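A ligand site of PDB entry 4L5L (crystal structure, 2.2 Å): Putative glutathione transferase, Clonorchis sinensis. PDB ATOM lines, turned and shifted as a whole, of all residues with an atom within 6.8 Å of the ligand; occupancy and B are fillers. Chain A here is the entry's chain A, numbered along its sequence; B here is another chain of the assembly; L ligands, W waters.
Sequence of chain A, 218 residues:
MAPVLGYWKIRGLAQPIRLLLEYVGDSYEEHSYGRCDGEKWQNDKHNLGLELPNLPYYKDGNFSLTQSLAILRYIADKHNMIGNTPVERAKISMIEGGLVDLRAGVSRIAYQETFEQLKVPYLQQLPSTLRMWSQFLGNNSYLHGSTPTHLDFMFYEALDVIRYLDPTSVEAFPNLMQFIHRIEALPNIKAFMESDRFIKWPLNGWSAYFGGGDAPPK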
ATOM      1  N   TYR A   7      31.545  30.360  36.153  1.00  0.00           N
ATOM      2  CA  TYR A   7      31.562  29.438  35.044  1.00  0.00           C
ATOM      3  C   TYR A   7      32.096  28.051  35.413  1.00  0.00           C
ATOM      4  O   TYR A   7      32.695  27.826  36.469  1.00  0.00           O
ATOM      5  CB  TYR A   7      32.410  29.997  33.895  1.00  0.00           C
ATOM      6  CG  TYR A   7      32.198  29.371  32.530  1.00  0.00           C
ATOM      7  CD1 TYR A   7      30.931  29.357  31.915  1.00  0.00           C
ATOM      8  CD2 TYR A   7      33.274  28.832  31.822  1.00  0.00           C
ATOM      9  CE1 TYR A   7      30.754  28.769  30.648  1.00  0.00           C
ATOM     10  CE2 TYR A   7      33.114  28.298  30.565  1.00  0.00           C
ATOM     11  CZ  TYR A   7      31.861  28.281  29.978  1.00  0.00           C
ATOM     12  OH  TYR A   7      31.762  27.712  28.778  1.00  0.00           O
ATOM     13  N   TRP A   8      31.835  27.095  34.542  1.00  0.00           N
ATOM     14  CA  TRP A   8      32.444  25.783  34.643  1.00  0.00           C
ATOM     15  C   TRP A   8      33.972  25.979  34.683  1.00  0.00           C
ATOM     16  O   TRP A   8      34.512  27.007  34.245  1.00  0.00           O
ATOM     17  CB  TRP A   8      32.007  24.888  33.505  1.00  0.00           C
ATOM     18  CG  TRP A   8      30.555  24.669  33.418  1.00  0.00           C
ATOM     19  CD1 TRP A   8      29.708  25.144  32.464  1.00  0.00           C
ATOM     20  CD2 TRP A   8      29.747  23.900  34.313  1.00  0.00           C
ATOM     21  NE1 TRP A   8      28.435  24.717  32.701  1.00  0.00           N
ATOM     22  CE2 TRP A   8      28.420  23.978  33.846  1.00  0.00           C
ATOM     23  CE3 TRP A   8      30.019  23.154  35.487  1.00  0.00           C
ATOM     24  CZ2 TRP A   8      27.351  23.343  34.484  1.00  0.00           C
ATOM     25  CZ3 TRP A   8      28.973  22.561  36.150  1.00  0.00           C
ATOM     26  CH2 TRP A   8      27.638  22.613  35.610  1.00  0.00           C
ATOM     27  N   ILE A  10      36.389  25.280  32.930  1.00  0.00           N
ATOM     28  CA  ILE A  10      36.803  24.935  31.584  1.00  0.00           C
ATOM     29  C   ILE A  10      37.144  26.263  30.908  1.00  0.00           C
ATOM     30  O   ILE A  10      36.858  27.304  31.438  1.00  0.00           O
ATOM     31  CB  ILE A  10      35.667  24.182  30.818  1.00  0.00           C
ATOM     32  CG1 ILE A  10      34.537  25.109  30.352  1.00  0.00           C
ATOM     33  CG2 ILE A  10      35.095  23.086  31.684  1.00  0.00           C
ATOM     34  CD1 ILE A  10      33.311  24.413  29.759  1.00  0.00           C
ATOM     35  N   GLY A  12      36.135  27.162  27.469  1.00  0.00           N
ATOM     36  CA  GLY A  12      34.871  27.472  26.829  1.00  0.00           C
ATOM     37  C   GLY A  12      34.653  28.945  26.519  1.00  0.00           C
ATOM     38  O   GLY A  12      35.540  29.601  26.034  1.00  0.00           O
ATOM     39  N   LEU A  13      33.479  29.435  26.899  1.00  0.00           N
ATOM     40  CA  LEU A  13      32.990  30.771  26.622  1.00  0.00           C
ATOM     41  C   LEU A  13      33.575  31.779  27.557  1.00  0.00           C
ATOM     42  O   LEU A  13      33.571  32.977  27.246  1.00  0.00           O
ATOM     43  CB  LEU A  13      31.450  30.815  26.741  1.00  0.00           C
ATOM     44  CG  LEU A  13      30.650  29.954  25.735  1.00  0.00           C
ATOM     45  CD1 LEU A  13      29.128  29.874  26.035  1.00  0.00           C
ATOM     46  CD2 LEU A  13      30.853  30.462  24.324  1.00  0.00           C
ATOM     47  N   TRP A  41      25.642  24.475  41.115  1.00  0.00           N
ATOM     48  CA  TRP A  41      25.165  25.403  40.073  1.00  0.00           C
ATOM     49  C   TRP A  41      23.642  25.426  40.071  1.00  0.00           C
ATOM     50  O   TRP A  41      23.033  26.493  39.958  1.00  0.00           O
ATOM     51  CB  TRP A  41      25.680  25.021  38.665  1.00  0.00           C
ATOM     52  CG  TRP A  41      24.899  25.712  37.584  1.00  0.00           C
ATOM     53  CD1 TRP A  41      24.259  25.111  36.557  1.00  0.00           C
ATOM     54  CD2 TRP A  41      24.671  27.116  37.433  1.00  0.00           C
ATOM     55  NE1 TRP A  41      23.630  26.026  35.780  1.00  0.00           N
ATOM     56  CE2 TRP A  41      23.851  27.279  36.303  1.00  0.00           C
ATOM     57  CE3 TRP A  41      25.029  28.259  38.164  1.00  0.00           C
ATOM     58  CZ2 TRP A  41      23.433  28.536  35.859  1.00  0.00           C
ATOM     59  CZ3 TRP A  41      24.583  29.494  37.749  1.00  0.00           C
ATOM     60  CH2 TRP A  41      23.816  29.620  36.599  1.00  0.00           C
ATOM     61  N   GLN A  42      23.004  24.283  40.180  1.00  0.00           N
ATOM     62  CA  GLN A  42      21.543  24.275  40.249  1.00  0.00           C
ATOM     63  C   GLN A  42      21.008  25.202  41.348  1.00  0.00           C
ATOM     64  O   GLN A  42      20.060  25.974  41.116  1.00  0.00           O
ATOM     65  CB  GLN A  42      20.953  22.867  40.366  1.00  0.00           C
ATOM     66  CG  GLN A  42      21.011  22.073  39.069  1.00  0.00           C
ATOM     67  CD  GLN A  42      20.589  22.845  37.826  1.00  0.00           C
ATOM     68  OE1 GLN A  42      19.471  23.340  37.715  1.00  0.00           O
ATOM     69  NE2 GLN A  42      21.474  22.926  36.849  1.00  0.00           N
ATOM     70  N   LYS A  45      21.803  28.913  40.482  1.00  0.00           N
ATOM     71  CA  LYS A  45      21.092  29.305  39.305  1.00  0.00           C
ATOM     72  C   LYS A  45      19.710  29.725  39.764  1.00  0.00           C
ATOM     73  O   LYS A  45      19.073  30.584  39.150  1.00  0.00           O
ATOM     74  CB  LYS A  45      21.009  28.137  38.354  1.00  0.00           C
ATOM     75  CG  LYS A  45      20.037  28.306  37.217  1.00  0.00           C
ATOM     76  CD  LYS A  45      20.094  27.169  36.173  1.00  0.00           C
ATOM     77  CE  LYS A  45      19.019  27.507  35.146  1.00  0.00           C
ATOM     78  NZ  LYS A  45      19.071  26.741  33.881  1.00  0.00           N
ATOM     79  N   PRO A  53      19.140  33.440  34.182  1.00  0.00           N
ATOM     80  CA  PRO A  53      20.155  32.558  34.753  1.00  0.00           C
ATOM     81  C   PRO A  53      20.860  31.758  33.663  1.00  0.00           C
ATOM     82  O   PRO A  53      20.231  31.256  32.782  1.00  0.00           O
ATOM     83  CB  PRO A  53      19.347  31.598  35.633  1.00  0.00           C
ATOM     84  CG  PRO A  53      18.136  32.368  36.044  1.00  0.00           C
ATOM     85  CD  PRO A  53      17.816  33.230  34.810  1.00  0.00           C
ATOM     86  N   ASN A  54      22.169  31.670  33.750  1.00  0.00           N
ATOM     87  CA  ASN A  54      22.986  30.958  32.784  1.00  0.00           C
ATOM     88  C   ASN A  54      24.421  31.002  33.296  1.00  0.00           C
ATOM     89  O   ASN A  54      24.740  31.744  34.245  1.00  0.00           O
ATOM     90  CB  ASN A  54      22.885  31.610  31.407  1.00  0.00           C
ATOM     91  CG  ASN A  54      22.811  30.589  30.290  1.00  0.00           C
ATOM     92  OD1 ASN A  54      23.365  29.500  30.399  1.00  0.00           O
ATOM     93  ND2 ASN A  54      22.152  30.939  29.216  1.00  0.00           N
ATOM     94  N   LEU A  55      25.267  30.224  32.665  1.00  0.00           N
ATOM     95  CA  LEU A  55      26.701  30.248  32.862  1.00  0.00           C
ATOM     96  C   LEU A  55      27.299  30.614  31.508  1.00  0.00           C
ATOM     97  O   LEU A  55      26.907  30.037  30.501  1.00  0.00           O
ATOM     98  CB  LEU A  55      27.219  28.879  33.295  1.00  0.00           C
ATOM     99  CG  LEU A  55      27.069  28.517  34.768  1.00  0.00           C
ATOM    100  CD1 LEU A  55      27.569  27.081  35.005  1.00  0.00           C
ATOM    101  CD2 LEU A  55      27.750  29.506  35.682  1.00  0.00           C
ATOM    102  N   PRO A  56      28.222  31.563  31.471  1.00  0.00           N
ATOM    103  CA  PRO A  56      28.751  32.303  32.615  1.00  0.00           C
ATOM    104  C   PRO A  56      27.838  33.406  33.156  1.00  0.00           C
ATOM    105  O   PRO A  56      26.942  33.838  32.476  1.00  0.00           O
ATOM    106  CB  PRO A  56      30.009  32.948  32.057  1.00  0.00           C
ATOM    107  CG  PRO A  56      29.666  33.159  30.621  1.00  0.00           C
ATOM    108  CD  PRO A  56      28.878  31.950  30.230  1.00  0.00           C
ATOM    109  N   THR A  66      24.145  37.907  32.663  1.00  0.00           N
ATOM    110  CA  THR A  66      24.518  36.676  32.000  1.00  0.00           C
ATOM    111  C   THR A  66      24.823  36.935  30.530  1.00  0.00           C
ATOM    112  O   THR A  66      24.699  38.069  30.056  1.00  0.00           O
ATOM    113  CB  THR A  66      23.499  35.566  32.229  1.00  0.00           C
ATOM    114  OG1 THR A  66      22.245  35.979  31.793  1.00  0.00           O
ATOM    115  CG2 THR A  66      23.413  35.205  33.702  1.00  0.00           C
ATOM    116  N   GLN A  67      25.259  35.878  29.821  1.00  0.00           N
ATOM    117  CA  GLN A  67      25.639  35.908  28.379  1.00  0.00           C
ATOM    118  C   GLN A  67      27.076  36.348  28.202  1.00  0.00           C
ATOM    119  O   GLN A  67      27.424  37.504  28.419  1.00  0.00           O
ATOM    120  CB  GLN A  67      24.724  36.748  27.480  1.00  0.00           C
ATOM    121  CG  GLN A  67      23.299  36.227  27.346  1.00  0.00           C
ATOM    122  CD  GLN A  67      23.214  34.966  26.535  1.00  0.00           C
ATOM    123  OE1 GLN A  67      22.374  34.141  26.793  1.00  0.00           O
ATOM    124  NE2 GLN A  67      24.119  34.782  25.576  1.00  0.00           N
ATOM    125  N   SER A  68      27.936  35.410  27.809  1.00  0.00           N
ATOM    126  CA  SER A  68      29.330  35.660  27.542  1.00  0.00           C
ATOM    127  C   SER A  68      29.608  36.976  26.818  1.00  0.00           C
ATOM    128  O   SER A  68      30.474  37.727  27.243  1.00  0.00           O
ATOM    129  CB  SER A  68      29.977  34.445  26.803  1.00  0.00           C
ATOM    130  OG  SER A  68      29.390  34.226  25.525  1.00  0.00           O
ATOM    131  N   LEU A  69      28.897  37.274  25.738  1.00  0.00           N
ATOM    132  CA  LEU A  69      29.240  38.455  24.967  1.00  0.00           C
ATOM    133  C   LEU A  69      28.826  39.762  25.685  1.00  0.00           C
ATOM    134  O   LEU A  69      29.479  40.799  25.530  1.00  0.00           O
ATOM    135  CB  LEU A  69      28.529  38.436  23.606  1.00  0.00           C
ATOM    136  CG  LEU A  69      28.993  39.576  22.671  1.00  0.00           C
ATOM    137  CD1 LEU A  69      30.466  39.487  22.380  1.00  0.00           C
ATOM    138  CD2 LEU A  69      28.234  39.481  21.373  1.00  0.00           C
ATOM    139  N   ALA A  70      27.730  39.702  26.434  1.00  0.00           N
ATOM    140  CA  ALA A  70      27.266  40.820  27.236  1.00  0.00           C
ATOM    141  C   ALA A  70      28.295  41.084  28.322  1.00  0.00           C
ATOM    142  O   ALA A  70      28.663  42.219  28.526  1.00  0.00           O
ATOM    143  CB  ALA A  70      25.898  40.523  27.849  1.00  0.00           C
ATOM    144  N   ILE A  71      28.813  40.039  28.968  1.00  0.00           N
ATOM    145  CA  ILE A  71      29.793  40.232  30.036  1.00  0.00           C
ATOM    146  C   ILE A  71      31.112  40.748  29.438  1.00  0.00           C
ATOM    147  O   ILE A  71      31.680  41.733  29.946  1.00  0.00           O
ATOM    148  CB  ILE A  71      30.100  38.970  30.797  1.00  0.00           C
ATOM    149  CG1 ILE A  71      28.832  38.418  31.418  1.00  0.00           C
ATOM    150  CG2 ILE A  71      31.172  39.209  31.875  1.00  0.00           C
ATOM    151  CD1 ILE A  71      28.892  36.962  31.887  1.00  0.00           C
ATOM    152  N   TYR A 111      31.076  18.019  20.648  1.00  0.00           N
ATOM    153  CA  TYR A 111      30.336  17.145  21.562  1.00  0.00           C
ATOM    154  C   TYR A 111      29.787  15.906  20.869  1.00  0.00           C
ATOM    155  O   TYR A 111      29.183  15.070  21.516  1.00  0.00           O
ATOM    156  CB  TYR A 111      29.190  17.878  22.277  1.00  0.00           C
ATOM    157  CG  TYR A 111      29.715  19.027  23.106  1.00  0.00           C
ATOM    158  CD1 TYR A 111      29.916  20.294  22.551  1.00  0.00           C
ATOM    159  CD2 TYR A 111      30.096  18.823  24.442  1.00  0.00           C
ATOM    160  CE1 TYR A 111      30.425  21.343  23.306  1.00  0.00           C
ATOM    161  CE2 TYR A 111      30.630  19.824  25.196  1.00  0.00           C
ATOM    162  CZ  TYR A 111      30.800  21.085  24.624  1.00  0.00           C
ATOM    163  OH  TYR A 111      31.349  22.018  25.418  1.00  0.00           O
ATOM    164  N   GLY B  97      21.431  38.212  23.780  1.00  0.00           N
ATOM    165  CA  GLY B  97      22.103  36.913  23.778  1.00  0.00           C
ATOM    166  C   GLY B  97      21.180  35.823  24.225  1.00  0.00           C
ATOM    167  O   GLY B  97      21.158  34.772  23.592  1.00  0.00           O
ATOM    168  N   GLY B  98      20.358  36.088  25.246  1.00  0.00           N
ATOM    169  CA  GLY B  98      19.266  35.189  25.632  1.00  0.00           C
ATOM    170  C   GLY B  98      18.297  34.872  24.485  1.00  0.00           C
ATOM    171  O   GLY B  98      17.879  33.698  24.279  1.00  0.00           O
ATOM    172  N   VAL B 100      18.886  35.303  21.217  1.00  0.00           N
ATOM    173  CA  VAL B 100      19.666  34.524  20.238  1.00  0.00           C
ATOM    174  C   VAL B 100      19.584  33.035  20.591  1.00  0.00           C
ATOM    175  O   VAL B 100      19.269  32.248  19.730  1.00  0.00           O
ATOM    176  CB  VAL B 100      21.117  35.016  20.101  1.00  0.00           C
ATOM    177  CG1 VAL B 100      22.018  34.021  19.381  1.00  0.00           C
ATOM    178  CG2 VAL B 100      21.208  36.369  19.332  1.00  0.00           C
ATOM    179  N   ASP B 101      19.890  32.668  21.835  1.00  0.00           N
ATOM    180  CA  ASP B 101      19.725  31.275  22.330  1.00  0.00           C
ATOM    181  C   ASP B 101      18.308  30.728  22.178  1.00  0.00           C
ATOM    182  O   ASP B 101      18.123  29.582  21.768  1.00  0.00           O
ATOM    183  CB  ASP B 101      20.111  31.143  23.847  1.00  0.00           C
ATOM    184  CG  ASP B 101      21.610  31.460  24.092  1.00  0.00           C
ATOM    185  OD1 ASP B 101      22.367  31.453  23.130  1.00  0.00           O
ATOM    186  OD2 ASP B 101      22.024  31.684  25.243  1.00  0.00           O
ATOM    187  N   ARG B 108      19.020  24.518  16.169  1.00  0.00           N
ATOM    188  CA  ARG B 108      19.944  23.445  16.496  1.00  0.00           C
ATOM    189  C   ARG B 108      19.319  22.099  16.098  1.00  0.00           C
ATOM    190  O   ARG B 108      20.014  21.234  15.615  1.00  0.00           O
ATOM    191  CB  ARG B 108      20.298  23.407  18.013  1.00  0.00           C
ATOM    192  CG  ARG B 108      21.667  23.975  18.384  1.00  0.00           C
ATOM    193  CD  ARG B 108      22.071  23.806  19.870  1.00  0.00           C
ATOM    194  NE  ARG B 108      21.353  24.743  20.740  1.00  0.00           N
ATOM    195  CZ  ARG B 108      21.604  26.063  20.821  1.00  0.00           C
ATOM    196  NH1 ARG B 108      22.551  26.619  20.059  1.00  0.00           N
ATOM    197  NH2 ARG B 108      20.879  26.845  21.641  1.00  0.00           N
HETATM  198  N1  LIG L   1      24.852  32.087  24.715  1.00  0.00           N
HETATM  199  C1  LIG L   1      25.302  31.820  26.034  1.00  0.00           C
HETATM  200  C2  LIG L   1      26.511  32.602  26.359  1.00  0.00           C
HETATM  201  O1  LIG L   1      27.218  33.037  25.443  1.00  0.00           O
HETATM  202  O2  LIG L   1      26.685  32.818  27.573  1.00  0.00           O
HETATM  203  C3  LIG L   1      25.540  30.339  26.184  1.00  0.00           C
HETATM  204  C4  LIG L   1      25.654  29.952  27.641  1.00  0.00           C
HETATM  205  C5  LIG L   1      25.451  28.452  27.827  1.00  0.00           C
HETATM  206  O3  LIG L   1      24.935  27.787  26.943  1.00  0.00           O
HETATM  207  N2  LIG L   1      25.966  27.929  28.948  1.00  0.00           N
HETATM  208  C6  LIG L   1      26.131  26.536  29.242  1.00  0.00           C
HETATM  209  C7  LIG L   1      25.562  26.217  30.606  1.00  0.00           C
HETATM  210  O4  LIG L   1      26.089  25.375  31.337  1.00  0.00           O
HETATM  211  C8  LIG L   1      27.617  26.291  29.246  1.00  0.00           C
HETATM  212  S1  LIG L   1      28.600  26.885  27.815  1.00  0.00           S
HETATM  213  N3  LIG L   1      24.516  26.993  30.962  1.00  0.00           N
HETATM  214  C9  LIG L   1      23.858  26.960  32.225  1.00  0.00           C
HETATM  215  C10 LIG L   1      22.708  25.994  32.282  1.00  0.00           C
HETATM  216  O5  LIG L   1      22.542  25.246  31.296  1.00  0.00           O
HETATM  217  O6  LIG L   1      21.981  25.942  33.316  1.00  0.00           O
HETATM  218  O   HOH W   1      25.557  33.117  30.198  1.00  0.00           O
HETATM  219  O   HOH W   2      26.416  35.911  24.325  1.00  0.00           O
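O6 of the ligand lies within hydrogen-bond range of NE1 of Trp 41 (3.0 Å).
The side-chain hydroxyl (OH) of Tyr 7 lies close to a sulfur (S1) of the ligand (3.4 Å).
The backbone carbonyl oxygen (O) of Leu 55 is in hydrogen-bond range of a nitrogen (N2) of the ligand, 2.8 Å away.
A nitrogen (N1) of the ligand sits close to the side-chain amide nitrogen (NE2) of Gln 67, 2.9 Å away.
O2 of the ligand is in hydrogen-bond range of N of Ser 68 (2.9 Å).
The side-chain hydroxyl of Ser 68 is in hydrogen-bond range of an oxygen (O1) of the ligand (2.5 Å).
A nitrogen (N3) of the ligand is in hydrogen-bond range of the side-chain amide oxygen of Asn 54 (2.8 Å).
OD2 of Asp 101 of chain B lies within salt-bridge range of N1 of the ligand, 2.9 Å away.
The indole nitrogen (NE1) of Trp 8 lies within hydrogen-bond range of an oxygen (O4) of the ligand.
The side-chain amino group of Lys 45 is in salt-bridge range of an oxygen (O6) of the ligand.
The side-chain amide oxygen (OE1) of Gln 67 lies close to the backbone carbonyl oxygen (O) of Gly 97 of chain B (3.5 Å).
The side-chain amide oxygen (OE1) of Gln 67 lies close to the side-chain carboxylate (OD2) of Asp 101 of chain B.
OE1 of Gln 67 lies within hydrogen-bond range of N of Gly 98 of chain B (3.2 Å).
The backbone NH (N) of Leu 13 sits at hydrogen-bond distance from the side-chain hydroxyl (OH) of Tyr 7 (3.1 Å).
Water W1 lies within hydrogen-bond range of the backbone carbonyl oxygen (O) of Pro 56 (2.8 Å), the backbone NH (N) of Gln 67 (2.8 Å), an oxygen (O2) of the ligand (2.9 Å) and the backbone carbonyl oxygen (O) of Leu 55 (3.4 Å).
Water W2 lies within hydrogen-bond range of the side-chain amide nitrogen of Gln 67 (2.8 Å), the backbone NH of Leu 69 (3.2 Å) and an oxygen (O1) of the ligand (3.2 Å).
Merely in contact with the ligand: Leu 13 and Pro 56.
Hydrophobic or aromatic side chains within 4 Å of the ligand: Trp 8, Leu 13, Trp 41 and Pro 56.
Along chain A the residues within 4 Å of the ligand span positions 7 to 68.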
